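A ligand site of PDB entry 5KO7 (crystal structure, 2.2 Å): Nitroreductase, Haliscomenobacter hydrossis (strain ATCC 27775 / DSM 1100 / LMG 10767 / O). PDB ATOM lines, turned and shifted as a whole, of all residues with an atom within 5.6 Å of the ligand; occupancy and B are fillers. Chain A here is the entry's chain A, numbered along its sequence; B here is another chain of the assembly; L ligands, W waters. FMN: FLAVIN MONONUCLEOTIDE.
Water W5 lies within hydrogen-bond range of O1P of the ligand (2.5 Å), O of Thr 36 (2.7 Å) and NH2 of Arg 35 (2.8 Å). Water W3 lies within hydrogen-bond range of NE of Arg 212 (2.6 Å), O3P of the ligand (2.8 Å), O of Ala 60 of chain B (3.0 Å) and O of Thr 59 of chain B (3.3 Å). Water W2 bridges an oxygen (O2') of the ligand (2.9 Å) and the backbone NH (N) of Ala 64 of chain B (3.1 Å). Water W4 bridges the guanidinium group of Arg 38 (2.9 Å) and an oxygen (O4') of the ligand (3.2 Å). Water W1 lies within hydrogen-bond range of OG of Ser 62 of chain B (2.6 Å), ND1 of His 65 of chain B (3.0 Å) and O of Ala 60 of chain B (3.3 Å).
The backbone carbonyl oxygen (O) of Arg 34 sits at hydrogen-bond distance from the guanidinium group (NH2) of Arg 212, 2.6 Å away. The guanidinium group (NH2) of Arg 34 is in hydrogen-bond range of the backbone carbonyl oxygen (O) of Thr 59 of chain B, at 2.8 Å. NH2 of Arg 212 lies within hydrogen-bond range of O of Thr 59 of chain B. The backbone carbonyl oxygen of Tyr 146 of chain B lies within hydrogen-bond range of the side-chain hydroxyl of Ser 150 of chain B (2.7 Å). The backbone NH (N) of Gly 63 of chain B lies within hydrogen-bond range of the side-chain hydroxyl (OG) of Ser 150 of chain B (3.1 Å).
N10 of the ligand sits close to O of Thr 171. Leu 170 touches the ligand (CD1 to N1, 3.7 Å). His 172 touches the ligand. Leu 210 touches the ligand. CB of Pro 61 of chain B touches O3' of the ligand, at 3.0 Å. O of Ser 62 of chain B touches C2' of the ligand (3.4 Å). Gly 63 of chain B touches the ligand. His 65 of chain B touches the ligand (ND1 to C5', 3.5 Å). CB of Tyr 146 of chain B touches C7M of the ligand (3.7 Å). Glu 149 of chain B touches the ligand. Ser 150 of chain B touches the ligand (OG to C8M, 3.5 Å). Of the 24 residues printed, 17 come within 4 Å of the ligand.
An oxygen (O1P) of the ligand is in hydrogen-bond range of the backbone NH (N) of Thr 36 (2.6 Å). OG1 of Thr 36 sits at hydrogen-bond distance from O2P of the ligand (2.9 Å). The guanidinium group (NE) of Arg 38 sits at hydrogen-bond distance from an oxygen (O2) of the ligand, 2.8 Å away. NE of Arg 35 is in salt-bridge range of O1P of the ligand (2.9 Å). O2P of the ligand lies within salt-bridge range of NH2 of Arg 34 (2.9 Å). An oxygen (O3P) of the ligand is in salt-bridge range of the guanidinium group (NH2) of Arg 212 (3.1 Å). The backbone NH (N) of Thr 173 sits close to an oxygen (O4) of the ligand, 3.4 Å away.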
ATOM      1  N   ARG A  34       9.574  20.515  -2.444  1.00  0.00           N
ATOM      2  CA  ARG A  34       9.615  20.360  -0.987  1.00  0.00           C
ATOM      3  C   ARG A  34       8.310  19.770  -0.484  1.00  0.00           C
ATOM      4  O   ARG A  34       7.225  20.215  -0.857  1.00  0.00           O
ATOM      5  CB  ARG A  34       9.867  21.700  -0.303  1.00  0.00           C
ATOM      6  CG  ARG A  34      10.011  21.613   1.219  1.00  0.00           C
ATOM      7  CD  ARG A  34       9.560  22.897   1.907  1.00  0.00           C
ATOM      8  NE  ARG A  34       8.128  23.137   1.747  1.00  0.00           N
ATOM      9  CZ  ARG A  34       7.174  22.460   2.380  1.00  0.00           C
ATOM     10  NH1 ARG A  34       7.482  21.477   3.217  1.00  0.00           N
ATOM     11  NH2 ARG A  34       5.888  22.757   2.171  1.00  0.00           N
ATOM     12  N   ARG A  35       8.417  18.775   0.385  1.00  0.00           N
ATOM     13  CA  ARG A  35       7.245  18.197   1.030  1.00  0.00           C
ATOM     14  C   ARG A  35       7.558  17.889   2.479  1.00  0.00           C
ATOM     15  O   ARG A  35       8.664  17.484   2.815  1.00  0.00           O
ATOM     16  CB  ARG A  35       6.781  16.937   0.302  1.00  0.00           C
ATOM     17  CG  ARG A  35       6.206  17.177  -1.093  1.00  0.00           C
ATOM     18  CD  ARG A  35       4.965  18.064  -1.047  1.00  0.00           C
ATOM     19  NE  ARG A  35       3.996  17.586  -0.061  1.00  0.00           N
ATOM     20  CZ  ARG A  35       3.105  16.631  -0.292  1.00  0.00           C
ATOM     21  NH1 ARG A  35       3.049  16.044  -1.482  1.00  0.00           N
ATOM     22  NH2 ARG A  35       2.259  16.262   0.661  1.00  0.00           N
ATOM     23  N   THR A  36       6.574  18.083   3.354  1.00  0.00           N
ATOM     24  CA  THR A  36       6.699  17.676   4.741  1.00  0.00           C
ATOM     25  C   THR A  36       6.770  16.163   4.806  1.00  0.00           C
ATOM     26  O   THR A  36       5.894  15.471   4.298  1.00  0.00           O
ATOM     27  CB  THR A  36       5.512  18.193   5.597  1.00  0.00           C
ATOM     28  OG1 THR A  36       5.621  19.615   5.749  1.00  0.00           O
ATOM     29  CG2 THR A  36       5.525  17.554   6.984  1.00  0.00           C
ATOM     30  N   ARG A  38       7.298  12.715   7.325  1.00  0.00           N
ATOM     31  CA  ARG A  38       6.984  12.309   8.687  1.00  0.00           C
ATOM     32  C   ARG A  38       7.652  10.979   9.056  1.00  0.00           C
ATOM     33  O   ARG A  38       7.488  10.491  10.175  1.00  0.00           O
ATOM     34  CB  ARG A  38       5.470  12.212   8.874  1.00  0.00           C
ATOM     35  CG  ARG A  38       4.752  13.521   8.606  1.00  0.00           C
ATOM     36  CD  ARG A  38       3.280  13.459   8.978  1.00  0.00           C
ATOM     37  NE  ARG A  38       2.651  14.769   8.893  1.00  0.00           N
ATOM     38  CZ  ARG A  38       2.291  15.348   7.745  1.00  0.00           C
ATOM     39  NH1 ARG A  38       2.496  14.740   6.591  1.00  0.00           N
ATOM     40  NH2 ARG A  38       1.719  16.545   7.770  1.00  0.00           N
ATOM     41  N   GLU A  91      -1.203  14.982  22.818  1.00  0.00           N
ATOM     42  CA  GLU A  91      -2.036  14.765  21.645  1.00  0.00           C
ATOM     43  C   GLU A  91      -2.963  13.563  21.872  1.00  0.00           C
ATOM     44  O   GLU A  91      -4.013  13.456  21.235  1.00  0.00           O
ATOM     45  CB  GLU A  91      -1.171  14.542  20.397  1.00  0.00           C
ATOM     46  CG  GLU A  91      -1.975  14.308  19.123  1.00  0.00           C
ATOM     47  CD  GLU A  91      -1.227  14.743  17.877  1.00  0.00           C
ATOM     48  OE1 GLU A  91      -1.353  14.063  16.840  1.00  0.00           O
ATOM     49  OE2 GLU A  91      -0.515  15.773  17.929  1.00  0.00           O
ATOM     50  N   LEU A 170       9.724  18.087   9.437  1.00  0.00           N
ATOM     51  CA  LEU A 170       8.315  18.033   9.804  1.00  0.00           C
ATOM     52  C   LEU A 170       7.950  19.243  10.643  1.00  0.00           C
ATOM     53  O   LEU A 170       8.082  19.217  11.859  1.00  0.00           O
ATOM     54  CB  LEU A 170       8.005  16.739  10.552  1.00  0.00           C
ATOM     55  CG  LEU A 170       6.643  16.620  11.237  1.00  0.00           C
ATOM     56  CD1 LEU A 170       5.500  17.028  10.314  1.00  0.00           C
ATOM     57  CD2 LEU A 170       6.420  15.197  11.739  1.00  0.00           C
ATOM     58  N   THR A 171       7.520  20.312   9.994  1.00  0.00           N
ATOM     59  CA  THR A 171       7.022  21.475  10.708  1.00  0.00           C
ATOM     60  C   THR A 171       5.919  21.009  11.648  1.00  0.00           C
ATOM     61  O   THR A 171       4.898  20.502  11.196  1.00  0.00           O
ATOM     62  CB  THR A 171       6.494  22.559   9.759  1.00  0.00           C
ATOM     63  OG1 THR A 171       7.493  22.868   8.783  1.00  0.00           O
ATOM     64  CG2 THR A 171       6.138  23.819  10.527  1.00  0.00           C
ATOM     65  N   HIS A 172       6.155  21.159  12.948  1.00  0.00           N
ATOM     66  CA  HIS A 172       5.271  20.595  13.962  1.00  0.00           C
ATOM     67  C   HIS A 172       4.915  21.629  15.015  1.00  0.00           C
ATOM     68  O   HIS A 172       5.705  22.523  15.314  1.00  0.00           O
ATOM     69  CB  HIS A 172       5.938  19.380  14.615  1.00  0.00           C
ATOM     70  CG  HIS A 172       4.976  18.477  15.332  1.00  0.00           C
ATOM     71  ND1 HIS A 172       4.655  17.216  14.886  1.00  0.00           N
ATOM     72  CD2 HIS A 172       4.273  18.652  16.478  1.00  0.00           C
ATOM     73  CE1 HIS A 172       3.797  16.662  15.710  1.00  0.00           C
ATOM     74  NE2 HIS A 172       3.540  17.513  16.688  1.00  0.00           N
ATOM     75  N   THR A 173       3.725  21.498  15.589  1.00  0.00           N
ATOM     76  CA  THR A 173       3.277  22.400  16.649  1.00  0.00           C
ATOM     77  C   THR A 173       4.197  22.305  17.858  1.00  0.00           C
ATOM     78  O   THR A 173       4.653  21.222  18.220  1.00  0.00           O
ATOM     79  CB  THR A 173       1.838  22.076  17.089  1.00  0.00           C
ATOM     80  OG1 THR A 173       1.797  20.775  17.671  1.00  0.00           O
ATOM     81  CG2 THR A 173       0.891  22.129  15.902  1.00  0.00           C
ATOM     82  N   LEU A 194       7.876  26.840  17.304  1.00  0.00           N
ATOM     83  CA  LEU A 194       7.723  25.709  16.392  1.00  0.00           C
ATOM     84  C   LEU A 194       8.655  24.556  16.725  1.00  0.00           C
ATOM     85  O   LEU A 194       9.780  24.757  17.199  1.00  0.00           O
ATOM     86  CB  LEU A 194       7.994  26.154  14.948  1.00  0.00           C
ATOM     87  CG  LEU A 194       6.761  26.547  14.122  1.00  0.00           C
ATOM     88  CD1 LEU A 194       7.177  27.169  12.815  1.00  0.00           C
ATOM     89  CD2 LEU A 194       5.891  25.335  13.877  1.00  0.00           C
ATOM     90  N   LEU A 210      -1.061  15.449  -2.013  1.00  0.00           N
ATOM     91  CA  LEU A 210      -1.709  16.749  -1.854  1.00  0.00           C
ATOM     92  C   LEU A 210      -1.521  17.619  -3.083  1.00  0.00           C
ATOM     93  O   LEU A 210      -0.559  17.444  -3.841  1.00  0.00           O
ATOM     94  CB  LEU A 210      -1.161  17.473  -0.625  1.00  0.00           C
ATOM     95  CG  LEU A 210      -1.402  16.807   0.735  1.00  0.00           C
ATOM     96  CD1 LEU A 210      -0.684  17.582   1.835  1.00  0.00           C
ATOM     97  CD2 LEU A 210      -2.891  16.708   1.037  1.00  0.00           C
ATOM     98  N   ARG A 212      -1.417  21.745  -4.224  1.00  0.00           N
ATOM     99  CA  ARG A 212      -1.319  23.120  -3.759  1.00  0.00           C
ATOM    100  C   ARG A 212      -2.219  24.022  -4.600  1.00  0.00           C
ATOM    101  O   ARG A 212      -2.449  23.750  -5.776  1.00  0.00           O
ATOM    102  CB  ARG A 212       0.130  23.599  -3.813  1.00  0.00           C
ATOM    103  CG  ARG A 212       1.073  22.778  -2.961  1.00  0.00           C
ATOM    104  CD  ARG A 212       2.418  23.468  -2.785  1.00  0.00           C
ATOM    105  NE  ARG A 212       3.202  22.824  -1.740  1.00  0.00           N
ATOM    106  CZ  ARG A 212       4.350  22.187  -1.943  1.00  0.00           C
ATOM    107  NH1 ARG A 212       4.875  22.119  -3.159  1.00  0.00           N
ATOM    108  NH2 ARG A 212       4.991  21.628  -0.918  1.00  0.00           N
ATOM    109  N   THR B  59       4.204  27.585  -1.695  1.00  0.00           N
ATOM    110  CA  THR B  59       4.607  26.195  -1.468  1.00  0.00           C
ATOM    111  C   THR B  59       4.918  25.945  -0.001  1.00  0.00           C
ATOM    112  O   THR B  59       5.221  24.817   0.392  1.00  0.00           O
ATOM    113  CB  THR B  59       5.854  25.804  -2.292  1.00  0.00           C
ATOM    114  OG1 THR B  59       6.980  26.569  -1.860  1.00  0.00           O
ATOM    115  CG2 THR B  59       5.607  26.025  -3.774  1.00  0.00           C
ATOM    116  N   ALA B  60       4.854  26.987   0.816  1.00  0.00           N
ATOM    117  CA  ALA B  60       5.148  26.861   2.238  1.00  0.00           C
ATOM    118  C   ALA B  60       4.207  25.860   2.904  1.00  0.00           C
ATOM    119  O   ALA B  60       3.076  25.669   2.449  1.00  0.00           O
ATOM    120  CB  ALA B  60       5.036  28.200   2.926  1.00  0.00           C
ATOM    121  N   PRO B  61       4.667  25.214   3.980  1.00  0.00           N
ATOM    122  CA  PRO B  61       3.745  24.359   4.733  1.00  0.00           C
ATOM    123  C   PRO B  61       2.681  25.206   5.431  1.00  0.00           C
ATOM    124  O   PRO B  61       2.892  26.391   5.660  1.00  0.00           O
ATOM    125  CB  PRO B  61       4.662  23.659   5.742  1.00  0.00           C
ATOM    126  CG  PRO B  61       5.772  24.621   5.953  1.00  0.00           C
ATOM    127  CD  PRO B  61       5.996  25.275   4.619  1.00  0.00           C
ATOM    128  N   SER B  62       1.541  24.589   5.746  1.00  0.00           N
ATOM    129  CA  SER B  62       0.472  25.281   6.452  1.00  0.00           C
ATOM    130  C   SER B  62      -0.312  24.306   7.310  1.00  0.00           C
ATOM    131  O   SER B  62      -0.433  23.129   6.973  1.00  0.00           O
ATOM    132  CB  SER B  62      -0.463  25.982   5.468  1.00  0.00           C
ATOM    133  OG  SER B  62      -0.893  25.098   4.443  1.00  0.00           O
ATOM    134  N   GLY B  63      -0.843  24.805   8.417  1.00  0.00           N
ATOM    135  CA  GLY B  63      -1.679  23.999   9.275  1.00  0.00           C
ATOM    136  C   GLY B  63      -2.821  23.382   8.490  1.00  0.00           C
ATOM    137  O   GLY B  63      -3.642  24.093   7.903  1.00  0.00           O
ATOM    138  N   ALA B  64      -2.851  22.047   8.460  1.00  0.00           N
ATOM    139  CA  ALA B  64      -3.923  21.303   7.795  1.00  0.00           C
ATOM    140  C   ALA B  64      -3.993  21.565   6.287  1.00  0.00           C
ATOM    141  O   ALA B  64      -5.038  21.346   5.662  1.00  0.00           O
ATOM    142  CB  ALA B  64      -5.268  21.616   8.448  1.00  0.00           C
ATOM    143  N   HIS B  65      -2.891  22.011   5.702  1.00  0.00           N
ATOM    144  CA  HIS B  65      -2.809  22.279   4.262  1.00  0.00           C
ATOM    145  C   HIS B  65      -3.876  23.278   3.811  1.00  0.00           C
ATOM    146  O   HIS B  65      -4.312  23.263   2.655  1.00  0.00           O
ATOM    147  CB  HIS B  65      -2.948  20.968   3.471  1.00  0.00           C
ATOM    148  CG  HIS B  65      -2.607  21.103   2.026  1.00  0.00           C
ATOM    149  ND1 HIS B  65      -1.421  21.660   1.588  1.00  0.00           N
ATOM    150  CD2 HIS B  65      -3.290  20.755   0.906  1.00  0.00           C
ATOM    151  CE1 HIS B  65      -1.397  21.646   0.264  1.00  0.00           C
ATOM    152  NE2 HIS B  65      -2.520  21.101  -0.171  1.00  0.00           N
ATOM    153  N   TYR B 145      -5.818  26.702  11.002  1.00  0.00           N
ATOM    154  CA  TYR B 145      -4.938  26.255  12.062  1.00  0.00           C
ATOM    155  C   TYR B 145      -3.553  26.890  11.964  1.00  0.00           C
ATOM    156  O   TYR B 145      -2.917  26.829  10.910  1.00  0.00           O
ATOM    157  CB  TYR B 145      -4.810  24.728  12.034  1.00  0.00           C
ATOM    158  CG  TYR B 145      -6.121  24.013  12.226  1.00  0.00           C
ATOM    159  CD1 TYR B 145      -6.640  23.809  13.491  1.00  0.00           C
ATOM    160  CD2 TYR B 145      -6.833  23.530  11.133  1.00  0.00           C
ATOM    161  CE1 TYR B 145      -7.838  23.147  13.672  1.00  0.00           C
ATOM    162  CE2 TYR B 145      -8.036  22.867  11.298  1.00  0.00           C
ATOM    163  CZ  TYR B 145      -8.533  22.680  12.577  1.00  0.00           C
ATOM    164  OH  TYR B 145      -9.730  22.018  12.759  1.00  0.00           O
ATOM    165  N   TYR B 146      -3.106  27.483  13.060  1.00  0.00           N
ATOM    166  CA  TYR B 146      -1.782  28.093  13.154  1.00  0.00           C
ATOM    167  C   TYR B 146      -1.508  29.005  11.958  1.00  0.00           C
ATOM    168  O   TYR B 146      -0.557  28.809  11.206  1.00  0.00           O
ATOM    169  CB  TYR B 146      -0.711  27.016  13.260  1.00  0.00           C
ATOM    170  CG  TYR B 146      -0.803  26.234  14.548  1.00  0.00           C
ATOM    171  CD1 TYR B 146      -1.673  25.158  14.659  1.00  0.00           C
ATOM    172  CD2 TYR B 146      -0.052  26.591  15.654  1.00  0.00           C
ATOM    173  CE1 TYR B 146      -1.781  24.443  15.846  1.00  0.00           C
ATOM    174  CE2 TYR B 146      -0.154  25.898  16.843  1.00  0.00           C
ATOM    175  CZ  TYR B 146      -1.019  24.827  16.932  1.00  0.00           C
ATOM    176  OH  TYR B 146      -1.122  24.126  18.110  1.00  0.00           O
ATOM    177  N   GLU B 149       1.894  31.631  12.100  1.00  0.00           N
ATOM    178  CA  GLU B 149       3.169  30.988  11.791  1.00  0.00           C
ATOM    179  C   GLU B 149       3.189  30.458  10.368  1.00  0.00           C
ATOM    180  O   GLU B 149       4.212  30.529   9.695  1.00  0.00           O
ATOM    181  CB  GLU B 149       3.473  29.864  12.782  1.00  0.00           C
ATOM    182  CG  GLU B 149       2.273  29.104  13.323  1.00  0.00           C
ATOM    183  CD  GLU B 149       1.656  29.754  14.554  1.00  0.00           C
ATOM    184  OE1 GLU B 149       2.369  29.901  15.575  1.00  0.00           O
ATOM    185  OE2 GLU B 149       0.468  30.127  14.493  1.00  0.00           O
ATOM    186  N   SER B 150       2.066  29.911   9.908  1.00  0.00           N
ATOM    187  CA  SER B 150       1.958  29.410   8.541  1.00  0.00           C
ATOM    188  C   SER B 150       2.261  30.521   7.533  1.00  0.00           C
ATOM    189  O   SER B 150       3.100  30.348   6.641  1.00  0.00           O
ATOM    190  CB  SER B 150       0.554  28.851   8.278  1.00  0.00           C
ATOM    191  OG  SER B 150       0.344  27.634   8.980  1.00  0.00           O
ATOM    192  N   ILE B 153       5.890  31.803   7.812  1.00  0.00           N
ATOM    193  CA  ILE B 153       6.776  30.902   7.081  1.00  0.00           C
ATOM    194  C   ILE B 153       6.711  31.208   5.585  1.00  0.00           C
ATOM    195  O   ILE B 153       7.739  31.301   4.914  1.00  0.00           O
ATOM    196  CB  ILE B 153       6.409  29.419   7.328  1.00  0.00           C
ATOM    197  CG1 ILE B 153       6.812  29.019   8.749  1.00  0.00           C
ATOM    198  CG2 ILE B 153       7.113  28.499   6.337  1.00  0.00           C
ATOM    199  CD1 ILE B 153       6.227  27.684   9.199  1.00  0.00           C
HETATM  200  N1  FMN L   1       2.071  18.263  10.643  1.00  0.00           N
HETATM  201  C2  FMN L   1       1.814  17.290  11.587  1.00  0.00           C
HETATM  202  O2  FMN L   1       1.774  16.108  11.246  1.00  0.00           O
HETATM  203  N3  FMN L   1       1.597  17.644  12.899  1.00  0.00           N
HETATM  204  C4  FMN L   1       1.638  18.965  13.279  1.00  0.00           C
HETATM  205  O4  FMN L   1       1.445  19.270  14.452  1.00  0.00           O
HETATM  206  C4A FMN L   1       1.900  19.952  12.325  1.00  0.00           C
HETATM  207  N5  FMN L   1       1.941  21.273  12.706  1.00  0.00           N
HETATM  208  C5A FMN L   1       2.204  22.254  11.765  1.00  0.00           C
HETATM  209  C6  FMN L   1       2.245  23.577  12.170  1.00  0.00           C
HETATM  210  C7  FMN L   1       2.506  24.589  11.250  1.00  0.00           C
HETATM  211  C7M FMN L   1       2.527  26.012  11.731  1.00  0.00           C
HETATM  212  C8  FMN L   1       2.722  24.246   9.913  1.00  0.00           C
HETATM  213  C8M FMN L   1       3.010  25.297   8.887  1.00  0.00           C
HETATM  214  C9  FMN L   1       2.681  22.917   9.521  1.00  0.00           C
HETATM  215  C9A FMN L   1       2.420  21.905  10.440  1.00  0.00           C
HETATM  216  N10 FMN L   1       2.368  20.569  10.053  1.00  0.00           N
HETATM  217  C10 FMN L   1       2.117  19.589  11.002  1.00  0.00           C
HETATM  218  C1' FMN L   1       2.626  20.161   8.616  1.00  0.00           C
HETATM  219  C2' FMN L   1       1.436  20.440   7.707  1.00  0.00           C
HETATM  220  O2' FMN L   1       0.376  19.564   8.036  1.00  0.00           O
HETATM  221  C3' FMN L   1       1.868  20.293   6.249  1.00  0.00           C
HETATM  222  O3' FMN L   1       2.838  21.291   5.969  1.00  0.00           O
HETATM  223  C4' FMN L   1       0.686  20.367   5.287  1.00  0.00           C
HETATM  224  O4' FMN L   1      -0.035  19.161   5.389  1.00  0.00           O
HETATM  225  C5' FMN L   1       1.076  20.566   3.822  1.00  0.00           C
HETATM  226  O5' FMN L   1       2.049  19.626   3.435  1.00  0.00           O
HETATM  227  P   FMN L   1       3.426  20.101   2.746  1.00  0.00           P
HETATM  228  O1P FMN L   1       4.273  18.878   2.499  1.00  0.00           O
HETATM  229  O2P FMN L   1       4.148  21.030   3.690  1.00  0.00           O
HETATM  230  O3P FMN L   1       3.151  20.816   1.439  1.00  0.00           O
HETATM  231  O   HOH W   1       0.389  23.774   2.627  1.00  0.00           O
HETATM  232  O   HOH W   2      -1.227  20.270  10.407  1.00  0.00           O
HETATM  233  O   HOH W   3       2.315  23.370   0.653  1.00  0.00           O
HETATM  234  O   HOH W   4       1.663  16.647   4.501  1.00  0.00           O
HETATM  235  O   HOH W   5       3.725  16.478   3.031  1.00  0.00           O
